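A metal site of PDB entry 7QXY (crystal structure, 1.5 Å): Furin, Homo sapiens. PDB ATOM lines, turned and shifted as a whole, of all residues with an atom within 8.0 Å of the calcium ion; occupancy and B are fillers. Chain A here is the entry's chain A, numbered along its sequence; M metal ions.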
ATOM      1  N   PRO A   6     -20.496   6.709 -27.062  1.00  0.00           N
ATOM      2  CA  PRO A   6     -20.839   7.235 -25.737  1.00  0.00           C
ATOM      3  C   PRO A   6     -21.322   8.669 -25.740  1.00  0.00           C
ATOM      4  O   PRO A   6     -20.874   9.473 -26.549  1.00  0.00           O
ATOM      5  CB  PRO A   6     -19.518   7.124 -24.981  1.00  0.00           C
ATOM      6  CG  PRO A   6     -18.824   5.983 -25.624  1.00  0.00           C
ATOM      7  CD  PRO A   6     -19.131   6.134 -27.071  1.00  0.00           C
ATOM      8  N   THR A   7     -22.215   8.997 -24.811  1.00  0.00           N
ATOM      9  CA  THR A   7     -22.773  10.347 -24.679  1.00  0.00           C
ATOM     10  C   THR A   7     -22.142  11.113 -23.499  1.00  0.00           C
ATOM     11  O   THR A   7     -22.656  12.174 -23.142  1.00  0.00           O
ATOM     12  CB  THR A   7     -24.278  10.224 -24.461  1.00  0.00           C
ATOM     13  OG1 THR A   7     -24.489   9.423 -23.285  1.00  0.00           O
ATOM     14  CG2 THR A   7     -24.988   9.586 -25.642  1.00  0.00           C
ATOM     15  N   ASP A   8     -21.042  10.623 -22.902  1.00  0.00           N
ATOM     16  CA  ASP A   8     -20.446  11.278 -21.735  1.00  0.00           C
ATOM     17  C   ASP A   8     -20.043  12.712 -22.056  1.00  0.00           C
ATOM     18  O   ASP A   8     -19.643  12.986 -23.193  1.00  0.00           O
ATOM     19  CB  ASP A   8     -19.238  10.481 -21.213  1.00  0.00           C
ATOM     20  CG  ASP A   8     -19.640   9.075 -20.861  1.00  0.00           C
ATOM     21  OD1 ASP A   8     -20.126   8.364 -21.747  1.00  0.00           O
ATOM     22  OD2 ASP A   8     -19.483   8.695 -19.671  1.00  0.00           O
ATOM     23  N   PRO A   9     -20.135  13.636 -21.088  1.00  0.00           N
ATOM     24  CA  PRO A   9     -19.881  15.049 -21.407  1.00  0.00           C
ATOM     25  C   PRO A   9     -18.512  15.378 -21.975  1.00  0.00           C
ATOM     26  O   PRO A   9     -18.417  16.234 -22.846  1.00  0.00           O
ATOM     27  CB  PRO A   9     -20.129  15.781 -20.071  1.00  0.00           C
ATOM     28  CG  PRO A   9     -20.131  14.714 -19.017  1.00  0.00           C
ATOM     29  CD  PRO A   9     -20.612  13.477 -19.701  1.00  0.00           C
ATOM     30  N   LYS A  10     -17.462  14.687 -21.499  1.00  0.00           N
ATOM     31  CA  LYS A  10     -16.107  14.932 -21.971  1.00  0.00           C
ATOM     32  C   LYS A  10     -15.653  13.946 -23.059  1.00  0.00           C
ATOM     33  O   LYS A  10     -14.522  14.059 -23.521  1.00  0.00           O
ATOM     34  CB  LYS A  10     -15.120  14.910 -20.784  1.00  0.00           C
ATOM     35  CG  LYS A  10     -15.435  15.902 -19.656  1.00  0.00           C
ATOM     36  CD  LYS A  10     -15.185  17.344 -20.077  1.00  0.00           C
ATOM     37  CE  LYS A  10     -15.309  18.354 -18.958  1.00  0.00           C
ATOM     38  NZ  LYS A  10     -16.716  18.735 -18.696  1.00  0.00           N
ATOM     39  N   PHE A  11     -16.527  13.028 -23.530  1.00  0.00           N
ATOM     40  CA  PHE A  11     -16.148  12.094 -24.598  1.00  0.00           C
ATOM     41  C   PHE A  11     -15.726  12.836 -25.885  1.00  0.00           C
ATOM     42  O   PHE A  11     -14.702  12.441 -26.466  1.00  0.00           O
ATOM     43  CB  PHE A  11     -17.245  11.042 -24.866  1.00  0.00           C
ATOM     44  CG  PHE A  11     -16.939  10.191 -26.076  1.00  0.00           C
ATOM     45  CD1 PHE A  11     -15.905   9.278 -26.049  1.00  0.00           C
ATOM     46  CD2 PHE A  11     -17.619  10.388 -27.264  1.00  0.00           C
ATOM     47  CE1 PHE A  11     -15.584   8.534 -27.184  1.00  0.00           C
ATOM     48  CE2 PHE A  11     -17.318   9.622 -28.388  1.00  0.00           C
ATOM     49  CZ  PHE A  11     -16.288   8.721 -28.334  1.00  0.00           C
ATOM     50  N   GLN A  14     -12.039  13.501 -25.975  1.00  0.00           N
ATOM     51  CA  GLN A  14     -11.129  12.346 -26.003  1.00  0.00           C
ATOM     52  C   GLN A  14     -10.730  12.075 -27.437  1.00  0.00           C
ATOM     53  O   GLN A  14     -11.071  11.042 -28.012  1.00  0.00           O
ATOM     54  CB  GLN A  14     -11.815  11.137 -25.329  1.00  0.00           C
ATOM     55  CG  GLN A  14     -11.961  11.398 -23.840  1.00  0.00           C
ATOM     56  CD  GLN A  14     -12.562  10.303 -23.032  1.00  0.00           C
ATOM     57  OE1 GLN A  14     -13.687   9.864 -23.278  1.00  0.00           O
ATOM     58  NE2 GLN A  14     -11.852   9.836 -22.000  1.00  0.00           N
ATOM     59  N   HIS A  53     -14.795   6.720  -7.022  1.00  0.00           N
ATOM     60  CA  HIS A  53     -14.949   7.787  -8.007  1.00  0.00           C
ATOM     61  C   HIS A  53     -16.219   7.505  -8.825  1.00  0.00           C
ATOM     62  O   HIS A  53     -16.418   6.358  -9.211  1.00  0.00           O
ATOM     63  CB  HIS A  53     -13.735   7.862  -8.944  1.00  0.00           C
ATOM     64  CG  HIS A  53     -13.697   9.099  -9.770  1.00  0.00           C
ATOM     65  ND1 HIS A  53     -14.577   9.307 -10.812  1.00  0.00           N
ATOM     66  CD2 HIS A  53     -12.844  10.149  -9.696  1.00  0.00           C
ATOM     67  CE1 HIS A  53     -14.266  10.490 -11.323  1.00  0.00           C
ATOM     68  NE2 HIS A  53     -13.223  11.021 -10.691  1.00  0.00           N
ATOM     69  N   PRO A  54     -17.116   8.489  -9.054  1.00  0.00           N
ATOM     70  CA  PRO A  54     -18.353   8.191  -9.800  1.00  0.00           C
ATOM     71  C   PRO A  54     -18.141   7.608 -11.197  1.00  0.00           C
ATOM     72  O   PRO A  54     -19.057   6.953 -11.707  1.00  0.00           O
ATOM     73  CB  PRO A  54     -19.098   9.531  -9.829  1.00  0.00           C
ATOM     74  CG  PRO A  54     -18.099  10.559  -9.478  1.00  0.00           C
ATOM     75  CD  PRO A  54     -17.055   9.894  -8.634  1.00  0.00           C
ATOM     76  N   ASP A  55     -16.947   7.777 -11.817  1.00  0.00           N
ATOM     77  CA  ASP A  55     -16.689   7.149 -13.115  1.00  0.00           C
ATOM     78  C   ASP A  55     -15.875   5.859 -12.998  1.00  0.00           C
ATOM     79  O   ASP A  55     -15.613   5.268 -14.024  1.00  0.00           O
ATOM     80  CB  ASP A  55     -16.028   8.141 -14.107  1.00  0.00           C
ATOM     81  CG  ASP A  55     -16.703   8.222 -15.467  1.00  0.00           C
ATOM     82  OD1 ASP A  55     -17.885   7.821 -15.565  1.00  0.00           O
ATOM     83  OD2 ASP A  55     -16.049   8.656 -16.429  1.00  0.00           O
ATOM     84  N   LEU A  56     -15.513   5.396 -11.784  1.00  0.00           N
ATOM     85  CA  LEU A  56     -14.777   4.127 -11.619  1.00  0.00           C
ATOM     86  C   LEU A  56     -15.574   3.099 -10.811  1.00  0.00           C
ATOM     87  O   LEU A  56     -15.430   1.913 -11.060  1.00  0.00           O
ATOM     88  CB  LEU A  56     -13.431   4.354 -10.904  1.00  0.00           C
ATOM     89  CG  LEU A  56     -12.454   5.308 -11.598  1.00  0.00           C
ATOM     90  CD1 LEU A  56     -11.190   5.454 -10.769  1.00  0.00           C
ATOM     91  CD2 LEU A  56     -12.096   4.818 -13.003  1.00  0.00           C
ATOM     92  N   GLY A  93      -8.997   5.552 -15.009  1.00  0.00           N
ATOM     93  CA  GLY A  93     -10.036   6.113 -15.863  1.00  0.00           C
ATOM     94  C   GLY A  93      -9.727   5.974 -17.332  1.00  0.00           C
ATOM     95  O   GLY A  93     -10.619   5.770 -18.140  1.00  0.00           O
ATOM     96  N   ALA A  96     -10.715   2.173 -17.895  1.00  0.00           N
ATOM     97  CA  ALA A  96     -12.063   1.689 -17.694  1.00  0.00           C
ATOM     98  C   ALA A  96     -13.026   2.650 -17.028  1.00  0.00           C
ATOM     99  O   ALA A  96     -13.910   2.209 -16.287  1.00  0.00           O
ATOM    100  CB  ALA A  96     -11.973   0.391 -16.891  1.00  0.00           C
ATOM    101  N   ALA A  97     -12.959   3.956 -17.351  1.00  0.00           N
ATOM    102  CA  ALA A  97     -13.987   4.894 -16.855  1.00  0.00           C
ATOM    103  C   ALA A  97     -15.351   4.476 -17.462  1.00  0.00           C
ATOM    104  O   ALA A  97     -15.406   4.059 -18.623  1.00  0.00           O
ATOM    105  CB  ALA A  97     -13.673   6.313 -17.257  1.00  0.00           C
ATOM    106  N   VAL A  98     -16.397   4.493 -16.650  1.00  0.00           N
ATOM    107  CA  VAL A  98     -17.728   4.043 -17.055  1.00  0.00           C
ATOM    108  C   VAL A  98     -18.266   4.892 -18.189  1.00  0.00           C
ATOM    109  O   VAL A  98     -18.045   6.096 -18.201  1.00  0.00           O
ATOM    110  CB  VAL A  98     -18.667   4.078 -15.820  1.00  0.00           C
ATOM    111  CG1 VAL A  98     -20.123   3.809 -16.216  1.00  0.00           C
ATOM    112  CG2 VAL A  98     -18.208   3.078 -14.757  1.00  0.00           C
ATOM    113  N   ALA A  99     -19.004   4.279 -19.134  1.00  0.00           N
ATOM    114  CA  ALA A  99     -19.579   4.993 -20.260  1.00  0.00           C
ATOM    115  C   ALA A  99     -21.084   5.269 -20.052  1.00  0.00           C
ATOM    116  O   ALA A  99     -21.749   4.534 -19.324  1.00  0.00           O
ATOM    117  CB  ALA A  99     -19.394   4.172 -21.524  1.00  0.00           C
ATOM    118  N   ASN A 100     -21.602   6.289 -20.740  1.00  0.00           N
ATOM    119  CA  ASN A 100     -23.019   6.632 -20.758  1.00  0.00           C
ATOM    120  C   ASN A 100     -23.606   6.868 -19.365  1.00  0.00           C
ATOM    121  O   ASN A 100     -24.773   6.527 -19.125  1.00  0.00           O
ATOM    122  CB  ASN A 100     -23.784   5.543 -21.516  1.00  0.00           C
ATOM    123  CG  ASN A 100     -23.281   5.399 -22.934  1.00  0.00           C
ATOM    124  OD1 ASN A 100     -23.251   6.373 -23.691  1.00  0.00           O
ATOM    125  ND2 ASN A 100     -22.873   4.204 -23.331  1.00  0.00           N
ATOM    126  N   ASN A 101     -22.835   7.490 -18.468  1.00  0.00           N
ATOM    127  CA  ASN A 101     -23.300   7.760 -17.100  1.00  0.00           C
ATOM    128  C   ASN A 101     -23.305   9.265 -16.751  1.00  0.00           C
ATOM    129  O   ASN A 101     -23.439   9.606 -15.576  1.00  0.00           O
ATOM    130  CB  ASN A 101     -22.443   6.957 -16.097  1.00  0.00           C
ATOM    131  CG  ASN A 101     -21.016   7.440 -15.982  1.00  0.00           C
ATOM    132  OD1 ASN A 101     -20.475   8.071 -16.911  1.00  0.00           O
ATOM    133  ND2 ASN A 101     -20.378   7.198 -14.839  1.00  0.00           N
ATOM    134  N   GLY A 102     -23.169  10.144 -17.749  1.00  0.00           N
ATOM    135  CA  GLY A 102     -23.177  11.591 -17.530  1.00  0.00           C
ATOM    136  C   GLY A 102     -22.001  12.145 -16.748  1.00  0.00           C
ATOM    137  O   GLY A 102     -22.069  13.291 -16.291  1.00  0.00           O
ATOM    138  N   VAL A 103     -20.907  11.379 -16.617  1.00  0.00           N
ATOM    139  CA  VAL A 103     -19.752  11.804 -15.841  1.00  0.00           C
ATOM    140  C   VAL A 103     -18.506  11.707 -16.679  1.00  0.00           C
ATOM    141  O   VAL A 103     -18.281  10.683 -17.316  1.00  0.00           O
ATOM    142  CB  VAL A 103     -19.619  10.903 -14.577  1.00  0.00           C
ATOM    143  CG1 VAL A 103     -18.378  11.275 -13.764  1.00  0.00           C
ATOM    144  CG2 VAL A 103     -20.870  10.969 -13.711  1.00  0.00           C
ATOM    145  N   CYS A 104     -17.680  12.761 -16.667  1.00  0.00           N
ATOM    146  CA  CYS A 104     -16.369  12.726 -17.293  1.00  0.00           C
ATOM    147  C   CYS A 104     -16.398  12.174 -18.762  1.00  0.00           C
ATOM    148  O   CYS A 104     -17.290  12.580 -19.516  1.00  0.00           O
ATOM    149  CB  CYS A 104     -15.439  11.924 -16.369  1.00  0.00           C
ATOM    150  SG  CYS A 104     -15.186  12.673 -14.739  1.00  0.00           S
ATOM    151  N   GLY A 105     -15.457  11.273 -19.166  1.00  0.00           N
ATOM    152  CA  GLY A 105     -15.440  10.646 -20.472  1.00  0.00           C
ATOM    153  C   GLY A 105     -15.639   9.155 -20.313  1.00  0.00           C
ATOM    154  O   GLY A 105     -16.396   8.709 -19.435  1.00  0.00           O
ATOM    155  N   VAL A 106     -14.921   8.357 -21.106  1.00  0.00           N
ATOM    156  CA  VAL A 106     -15.020   6.903 -21.049  1.00  0.00           C
ATOM    157  C   VAL A 106     -13.621   6.304 -21.093  1.00  0.00           C
ATOM    158  O   VAL A 106     -12.695   6.913 -21.624  1.00  0.00           O
ATOM    159  CB  VAL A 106     -15.855   6.336 -22.225  1.00  0.00           C
ATOM    160  CG1 VAL A 106     -17.193   7.023 -22.320  1.00  0.00           C
ATOM    161  CG2 VAL A 106     -15.101   6.435 -23.562  1.00  0.00           C
ATOM    162  N   GLY A 107     -13.514   5.070 -20.617  1.00  0.00           N
ATOM    163  CA  GLY A 107     -12.276   4.321 -20.743  1.00  0.00           C
ATOM    164  C   GLY A 107     -12.213   3.680 -22.112  1.00  0.00           C
ATOM    165  O   GLY A 107     -13.230   3.520 -22.797  1.00  0.00           O
ATOM    166  N   TYR A 110     -14.368   0.426 -21.523  1.00  0.00           N
ATOM    167  CA  TYR A 110     -15.330   0.976 -20.566  1.00  0.00           C
ATOM    168  C   TYR A 110     -16.233  -0.046 -19.860  1.00  0.00           C
ATOM    169  O   TYR A 110     -16.974   0.357 -18.953  1.00  0.00           O
ATOM    170  CB  TYR A 110     -16.177   2.081 -21.184  1.00  0.00           C
ATOM    171  CG  TYR A 110     -16.949   1.747 -22.440  1.00  0.00           C
ATOM    172  CD1 TYR A 110     -18.134   1.021 -22.384  1.00  0.00           C
ATOM    173  CD2 TYR A 110     -16.636   2.343 -23.651  1.00  0.00           C
ATOM    174  CE1 TYR A 110     -18.936   0.837 -23.500  1.00  0.00           C
ATOM    175  CE2 TYR A 110     -17.425   2.178 -24.785  1.00  0.00           C
ATOM    176  CZ  TYR A 110     -18.593   1.440 -24.698  1.00  0.00           C
ATOM    177  OH  TYR A 110     -19.376   1.287 -25.814  1.00  0.00           O
ATOM    178  N   THR A 247     -10.480  10.516 -15.325  1.00  0.00           N
ATOM    179  CA  THR A 247     -10.927  10.687 -13.952  1.00  0.00           C
ATOM    180  C   THR A 247      -9.792  11.238 -13.119  1.00  0.00           C
ATOM    181  O   THR A 247      -8.654  10.860 -13.323  1.00  0.00           O
ATOM    182  CB  THR A 247     -11.312   9.320 -13.366  1.00  0.00           C
ATOM    183  OG1 THR A 247     -10.283   8.365 -13.665  1.00  0.00           O
ATOM    184  CG2 THR A 247     -12.597   8.803 -13.941  1.00  0.00           C
HETATM  185 CA    CA M   1     -18.144   8.400 -17.807  1.00  0.00          CA
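The side-chain carboxylate (OD1) of Asp 8 is in hydrogen-bond range of the backbone NH (N) of Asn 100, 2.7 Å away.
The backbone NH (N) of Asp 55 sits at hydrogen-bond distance from a ring nitrogen (ND1) of His 53, 3.0 Å away.
The side-chain amide nitrogen of Asn 101 is in hydrogen-bond range of the backbone carbonyl oxygen of Pro 54 (3.4 Å).
The calcium ion is bound by the side-chain carboxylate (OD2) of Asp 8 (2.3 Å), the side-chain carboxylate (OD1) of Asp 55 (2.3 Å), the backbone carbonyl oxygen (O) of Val 103 (2.3 Å), the backbone carbonyl oxygen (O) of Val 98 (2.3 Å), the backbone carbonyl oxygen (O) of Gly 105 (2.4 Å), the side-chain amide oxygen (OD1) of Asn 101 (2.5 Å) and the side-chain carboxylate (OD2) of Asp 55 (2.5 Å).
Within 4 Å of the calcium ion: Asp 8, Asp 55, Val 98, Asn 101, Val 103 and Gly 105.
The nearest printed residue that does not touch the calcium ion is Cys 104 (4.3 Å).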
